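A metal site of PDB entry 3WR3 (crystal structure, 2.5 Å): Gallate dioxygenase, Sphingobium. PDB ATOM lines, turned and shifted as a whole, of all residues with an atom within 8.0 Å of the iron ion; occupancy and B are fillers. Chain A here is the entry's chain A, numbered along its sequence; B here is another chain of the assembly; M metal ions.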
ATOM      1  N   SER A  11      23.054  22.742  -0.141  1.00  0.00           N
ATOM      2  CA  SER A  11      23.432  21.357   0.107  1.00  0.00           C
ATOM      3  C   SER A  11      24.431  20.885  -0.941  1.00  0.00           C
ATOM      4  O   SER A  11      24.353  21.290  -2.098  1.00  0.00           O
ATOM      5  CB  SER A  11      22.196  20.442   0.098  1.00  0.00           C
ATOM      6  OG  SER A  11      21.168  20.948   0.929  1.00  0.00           O
ATOM      7  N   HIS A  12      25.387  20.056  -0.547  1.00  0.00           N
ATOM      8  CA  HIS A  12      26.126  19.306  -1.538  1.00  0.00           C
ATOM      9  C   HIS A  12      25.847  17.826  -1.302  1.00  0.00           C
ATOM     10  O   HIS A  12      25.853  17.358  -0.172  1.00  0.00           O
ATOM     11  CB  HIS A  12      27.634  19.641  -1.546  1.00  0.00           C
ATOM     12  CG  HIS A  12      28.345  19.424  -0.238  1.00  0.00           C
ATOM     13  ND1 HIS A  12      28.749  20.465   0.576  1.00  0.00           N
ATOM     14  CD2 HIS A  12      28.764  18.289   0.357  1.00  0.00           C
ATOM     15  CE1 HIS A  12      29.352  19.971   1.636  1.00  0.00           C
ATOM     16  NE2 HIS A  12      29.378  18.652   1.533  1.00  0.00           N
ATOM     17  N   THR A  13      25.552  17.116  -2.385  1.00  0.00           N
ATOM     18  CA  THR A  13      25.024  15.753  -2.372  1.00  0.00           C
ATOM     19  C   THR A  13      25.438  15.060  -3.655  1.00  0.00           C
ATOM     20  O   THR A  13      25.405  15.673  -4.721  1.00  0.00           O
ATOM     21  CB  THR A  13      23.473  15.770  -2.231  1.00  0.00           C
ATOM     22  OG1 THR A  13      23.082  16.489  -1.053  1.00  0.00           O
ATOM     23  CG2 THR A  13      22.923  14.384  -2.192  1.00  0.00           C
ATOM     24  N   PRO A  14      25.886  13.821  -3.555  1.00  0.00           N
ATOM     25  CA  PRO A  14      26.247  13.168  -4.812  1.00  0.00           C
ATOM     26  C   PRO A  14      25.017  12.771  -5.648  1.00  0.00           C
ATOM     27  O   PRO A  14      25.211  12.306  -6.756  1.00  0.00           O
ATOM     28  CB  PRO A  14      27.029  11.935  -4.355  1.00  0.00           C
ATOM     29  CG  PRO A  14      26.552  11.688  -2.944  1.00  0.00           C
ATOM     30  CD  PRO A  14      26.247  13.026  -2.368  1.00  0.00           C
ATOM     31  N   TYR A  56      33.675  23.962   1.589  1.00  0.00           N
ATOM     32  CA  TYR A  56      33.031  22.654   1.494  1.00  0.00           C
ATOM     33  C   TYR A  56      33.645  21.596   2.424  1.00  0.00           C
ATOM     34  O   TYR A  56      34.298  21.915   3.424  1.00  0.00           O
ATOM     35  CB  TYR A  56      33.063  22.175   0.034  1.00  0.00           C
ATOM     36  CG  TYR A  56      34.402  21.646  -0.446  1.00  0.00           C
ATOM     37  CD1 TYR A  56      34.545  20.319  -0.840  1.00  0.00           C
ATOM     38  CD2 TYR A  56      35.527  22.469  -0.509  1.00  0.00           C
ATOM     39  CE1 TYR A  56      35.758  19.829  -1.292  1.00  0.00           C
ATOM     40  CE2 TYR A  56      36.747  21.981  -0.949  1.00  0.00           C
ATOM     41  CZ  TYR A  56      36.859  20.663  -1.342  1.00  0.00           C
ATOM     42  OH  TYR A  56      38.069  20.162  -1.772  1.00  0.00           O
ATOM     43  N   ASN A  57      33.410  20.331   2.117  1.00  0.00           N
ATOM     44  CA  ASN A  57      33.932  19.237   2.910  1.00  0.00           C
ATOM     45  C   ASN A  57      34.286  18.103   1.974  1.00  0.00           C
ATOM     46  O   ASN A  57      33.433  17.625   1.216  1.00  0.00           O
ATOM     47  CB  ASN A  57      32.914  18.832   3.996  1.00  0.00           C
ATOM     48  CG  ASN A  57      32.981  17.349   4.374  1.00  0.00           C
ATOM     49  OD1 ASN A  57      33.850  16.922   5.145  1.00  0.00           O
ATOM     50  ND2 ASN A  57      32.045  16.576   3.861  1.00  0.00           N
ATOM     51  N   ASP A  58      35.549  17.714   1.970  1.00  0.00           N
ATOM     52  CA  ASP A  58      35.979  16.530   1.233  1.00  0.00           C
ATOM     53  C   ASP A  58      35.505  15.316   2.010  1.00  0.00           C
ATOM     54  O   ASP A  58      35.799  15.179   3.198  1.00  0.00           O
ATOM     55  CB  ASP A  58      37.501  16.528   1.040  1.00  0.00           C
ATOM     56  CG  ASP A  58      37.979  15.342   0.224  1.00  0.00           C
ATOM     57  OD1 ASP A  58      38.027  15.473  -1.024  1.00  0.00           O
ATOM     58  OD2 ASP A  58      38.316  14.293   0.818  1.00  0.00           O
ATOM     59  N   HIS A  59      34.758  14.439   1.351  1.00  0.00           N
ATOM     60  CA  HIS A  59      34.195  13.263   2.024  1.00  0.00           C
ATOM     61  C   HIS A  59      35.156  12.088   1.910  1.00  0.00           C
ATOM     62  O   HIS A  59      34.809  11.024   1.361  1.00  0.00           O
ATOM     63  CB  HIS A  59      32.813  12.911   1.458  1.00  0.00           C
ATOM     64  CG  HIS A  59      31.831  14.027   1.588  1.00  0.00           C
ATOM     65  ND1 HIS A  59      31.861  15.137   0.762  1.00  0.00           N
ATOM     66  CD2 HIS A  59      30.826  14.241   2.465  1.00  0.00           C
ATOM     67  CE1 HIS A  59      30.891  15.958   1.114  1.00  0.00           C
ATOM     68  NE2 HIS A  59      30.243  15.442   2.136  1.00  0.00           N
ATOM     69  N   ASP A 123      35.941  16.689  -5.076  1.00  0.00           N
ATOM     70  CA  ASP A 123      34.939  15.642  -5.205  1.00  0.00           C
ATOM     71  C   ASP A 123      33.560  16.267  -5.243  1.00  0.00           C
ATOM     72  O   ASP A 123      33.423  17.452  -5.534  1.00  0.00           O
ATOM     73  CB  ASP A 123      35.092  14.597  -4.075  1.00  0.00           C
ATOM     74  CG  ASP A 123      34.838  15.158  -2.670  1.00  0.00           C
ATOM     75  OD1 ASP A 123      34.048  16.118  -2.484  1.00  0.00           O
ATOM     76  OD2 ASP A 123      35.421  14.600  -1.729  1.00  0.00           O
ATOM     77  N   HIS A 124      32.545  15.465  -4.941  1.00  0.00           N
ATOM     78  CA  HIS A 124      31.162  15.932  -5.013  1.00  0.00           C
ATOM     79  C   HIS A 124      30.892  17.020  -3.968  1.00  0.00           C
ATOM     80  O   HIS A 124      29.847  17.658  -4.005  1.00  0.00           O
ATOM     81  CB  HIS A 124      30.167  14.760  -4.833  1.00  0.00           C
ATOM     82  CG  HIS A 124      30.015  14.283  -3.417  1.00  0.00           C
ATOM     83  ND1 HIS A 124      30.602  13.123  -2.955  1.00  0.00           N
ATOM     84  CD2 HIS A 124      29.306  14.792  -2.379  1.00  0.00           C
ATOM     85  CE1 HIS A 124      30.273  12.948  -1.677  1.00  0.00           C
ATOM     86  NE2 HIS A 124      29.498  13.948  -1.305  1.00  0.00           N
ATOM     87  N   GLY A 125      31.844  17.243  -3.066  1.00  0.00           N
ATOM     88  CA  GLY A 125      31.682  18.276  -2.052  1.00  0.00           C
ATOM     89  C   GLY A 125      31.613  19.622  -2.729  1.00  0.00           C
ATOM     90  O   GLY A 125      30.949  20.554  -2.253  1.00  0.00           O
ATOM     91  N   VAL A 151      35.451  18.315   8.986  1.00  0.00           N
ATOM     92  CA  VAL A 151      34.311  18.133   9.875  1.00  0.00           C
ATOM     93  C   VAL A 151      34.036  16.659  10.210  1.00  0.00           C
ATOM     94  O   VAL A 151      33.184  16.374  11.041  1.00  0.00           O
ATOM     95  CB  VAL A 151      33.029  18.741   9.273  1.00  0.00           C
ATOM     96  CG1 VAL A 151      32.988  20.245   9.474  1.00  0.00           C
ATOM     97  CG2 VAL A 151      32.889  18.353   7.808  1.00  0.00           C
ATOM     98  N   LEU A 152      34.758  15.748   9.574  1.00  0.00           N
ATOM     99  CA  LEU A 152      34.459  14.312   9.662  1.00  0.00           C
ATOM    100  C   LEU A 152      35.202  13.552  10.766  1.00  0.00           C
ATOM    101  O   LEU A 152      34.707  12.550  11.268  1.00  0.00           O
ATOM    102  CB  LEU A 152      34.753  13.644   8.306  1.00  0.00           C
ATOM    103  CG  LEU A 152      33.931  14.134   7.104  1.00  0.00           C
ATOM    104  CD1 LEU A 152      34.288  13.361   5.848  1.00  0.00           C
ATOM    105  CD2 LEU A 152      32.430  14.050   7.403  1.00  0.00           C
ATOM    106  N   THR A 187      28.865  25.385   1.601  1.00  0.00           N
ATOM    107  CA  THR A 187      28.008  24.306   1.153  1.00  0.00           C
ATOM    108  C   THR A 187      27.817  23.252   2.254  1.00  0.00           C
ATOM    109  O   THR A 187      28.412  23.336   3.320  1.00  0.00           O
ATOM    110  CB  THR A 187      28.564  23.657  -0.142  1.00  0.00           C
ATOM    111  OG1 THR A 187      29.789  22.975   0.131  1.00  0.00           O
ATOM    112  CG2 THR A 187      28.776  24.712  -1.239  1.00  0.00           C
ATOM    113  N   GLY A 188      26.933  22.286   1.994  1.00  0.00           N
ATOM    114  CA  GLY A 188      26.653  21.232   2.955  1.00  0.00           C
ATOM    115  C   GLY A 188      25.250  21.280   3.521  1.00  0.00           C
ATOM    116  O   GLY A 188      24.452  22.158   3.163  1.00  0.00           O
ATOM    117  N   GLY A 189      24.954  20.327   4.405  1.00  0.00           N
ATOM    118  CA  GLY A 189      23.672  20.280   5.109  1.00  0.00           C
ATOM    119  C   GLY A 189      22.540  19.682   4.287  1.00  0.00           C
ATOM    120  O   GLY A 189      22.748  19.268   3.143  1.00  0.00           O
ATOM    121  N   HIS A 192      20.357  15.486   8.292  1.00  0.00           N
ATOM    122  CA  HIS A 192      20.414  14.132   7.805  1.00  0.00           C
ATOM    123  C   HIS A 192      21.457  13.303   8.575  1.00  0.00           C
ATOM    124  O   HIS A 192      22.367  13.841   9.210  1.00  0.00           O
ATOM    125  CB  HIS A 192      20.719  14.102   6.312  1.00  0.00           C
ATOM    126  CG  HIS A 192      22.146  14.399   5.982  1.00  0.00           C
ATOM    127  ND1 HIS A 192      22.718  15.643   6.177  1.00  0.00           N
ATOM    128  CD2 HIS A 192      23.119  13.614   5.453  1.00  0.00           C
ATOM    129  CE1 HIS A 192      23.983  15.601   5.789  1.00  0.00           C
ATOM    130  NE2 HIS A 192      24.246  14.393   5.347  1.00  0.00           N
ATOM    131  N   GLU A 236      25.907  13.567  10.479  1.00  0.00           N
ATOM    132  CA  GLU A 236      26.512  14.272   9.360  1.00  0.00           C
ATOM    133  C   GLU A 236      25.926  15.674   9.145  1.00  0.00           C
ATOM    134  O   GLU A 236      26.538  16.511   8.494  1.00  0.00           O
ATOM    135  CB  GLU A 236      26.382  13.450   8.071  1.00  0.00           C
ATOM    136  CG  GLU A 236      27.287  12.213   7.970  1.00  0.00           C
ATOM    137  CD  GLU A 236      26.784  11.011   8.797  1.00  0.00           C
ATOM    138  OE1 GLU A 236      25.827  11.139   9.594  1.00  0.00           O
ATOM    139  OE2 GLU A 236      27.356   9.909   8.623  1.00  0.00           O
ATOM    140  N   GLY A 237      24.746  15.925   9.692  1.00  0.00           N
ATOM    141  CA  GLY A 237      24.078  17.197   9.486  1.00  0.00           C
ATOM    142  C   GLY A 237      24.715  18.318  10.273  1.00  0.00           C
ATOM    143  O   GLY A 237      24.457  19.502  10.016  1.00  0.00           O
ATOM    144  N   GLU A 239      27.595  19.195   9.996  1.00  0.00           N
ATOM    145  CA  GLU A 239      28.535  19.818   9.075  1.00  0.00           C
ATOM    146  C   GLU A 239      28.070  21.215   8.642  1.00  0.00           C
ATOM    147  O   GLU A 239      28.800  21.927   7.951  1.00  0.00           O
ATOM    148  CB  GLU A 239      28.750  18.947   7.834  1.00  0.00           C
ATOM    149  CG  GLU A 239      27.701  19.188   6.748  1.00  0.00           C
ATOM    150  CD  GLU A 239      27.808  18.213   5.569  1.00  0.00           C
ATOM    151  OE1 GLU A 239      28.914  17.996   5.036  1.00  0.00           O
ATOM    152  OE2 GLU A 239      26.766  17.649   5.199  1.00  0.00           O
ATOM    153  N   VAL A 240      26.855  21.589   9.041  1.00  0.00           N
ATOM    154  CA  VAL A 240      26.359  22.962   8.860  1.00  0.00           C
ATOM    155  C   VAL A 240      27.111  23.950   9.738  1.00  0.00           C
ATOM    156  O   VAL A 240      26.638  25.057   9.985  1.00  0.00           O
ATOM    157  CB  VAL A 240      24.863  23.090   9.189  1.00  0.00           C
ATOM    158  CG1 VAL A 240      24.032  22.177   8.319  1.00  0.00           C
ATOM    159  CG2 VAL A 240      24.628  22.797  10.669  1.00  0.00           C
ATOM    160  N   MET A 242      29.798  24.815   8.562  1.00  0.00           N
ATOM    161  CA  MET A 242      30.266  25.498   7.364  1.00  0.00           C
ATOM    162  C   MET A 242      29.292  26.557   6.834  1.00  0.00           C
ATOM    163  O   MET A 242      29.639  27.313   5.916  1.00  0.00           O
ATOM    164  CB  MET A 242      30.548  24.466   6.291  1.00  0.00           C
ATOM    165  CG  MET A 242      31.597  23.459   6.706  1.00  0.00           C
ATOM    166  SD  MET A 242      32.063  22.442   5.321  1.00  0.00           S
ATOM    167  CE  MET A 242      30.683  21.296   5.288  1.00  0.00           C
ATOM    168  N   PHE B 374      31.600   7.193   4.241  1.00  0.00           N
ATOM    169  CA  PHE B 374      32.072   7.677   2.954  1.00  0.00           C
ATOM    170  C   PHE B 374      33.094   6.740   2.307  1.00  0.00           C
ATOM    171  O   PHE B 374      33.323   6.807   1.095  1.00  0.00           O
ATOM    172  CB  PHE B 374      32.650   9.060   3.134  1.00  0.00           C
ATOM    173  CG  PHE B 374      31.719   9.993   3.810  1.00  0.00           C
ATOM    174  CD1 PHE B 374      30.525  10.355   3.203  1.00  0.00           C
ATOM    175  CD2 PHE B 374      32.005  10.503   5.067  1.00  0.00           C
ATOM    176  CE1 PHE B 374      29.647  11.217   3.827  1.00  0.00           C
ATOM    177  CE2 PHE B 374      31.122  11.381   5.690  1.00  0.00           C
ATOM    178  CZ  PHE B 374      29.938  11.728   5.071  1.00  0.00           C
HETATM  179 FE    FE M   1      29.563  16.813   3.488  1.00  0.00          FE
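Along chain A the residues within 4 Å of the iron ion span positions 12 to 239. The nearest printed residue that does not touch the iron ion is Met 242 (5.0 Å).
The iron ion is bound by NE2 of His 59 (2.0 Å), OE1 of Glu 239 (2.1 Å) and ND2 of Asn 57 (2.5 Å). Slightly farther from the iron ion lies a ring nitrogen (NE2) of His 12 (2.7 Å).
N of His 59 lies within hydrogen-bond range of OD2 of Asp 123. A ring nitrogen (ND1) of His 12 is in hydrogen-bond range of the backbone NH (N) of Gly 188. A ring nitrogen (ND1) of His 12 sits at hydrogen-bond distance from the side-chain hydroxyl (OG1) of Thr 187 (2.8 Å). The backbone NH of Gly 189 lies within hydrogen-bond range of the side-chain carboxylate of Glu 239 (3.3 Å). A ring nitrogen (NE2) of His 12 sits close to a ring nitrogen (NE2) of His 59, 3.4 Å away. A ring nitrogen (ND1) of His 59 lies within hydrogen-bond range of a ring nitrogen (NE2) of His 124 (3.4 Å).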
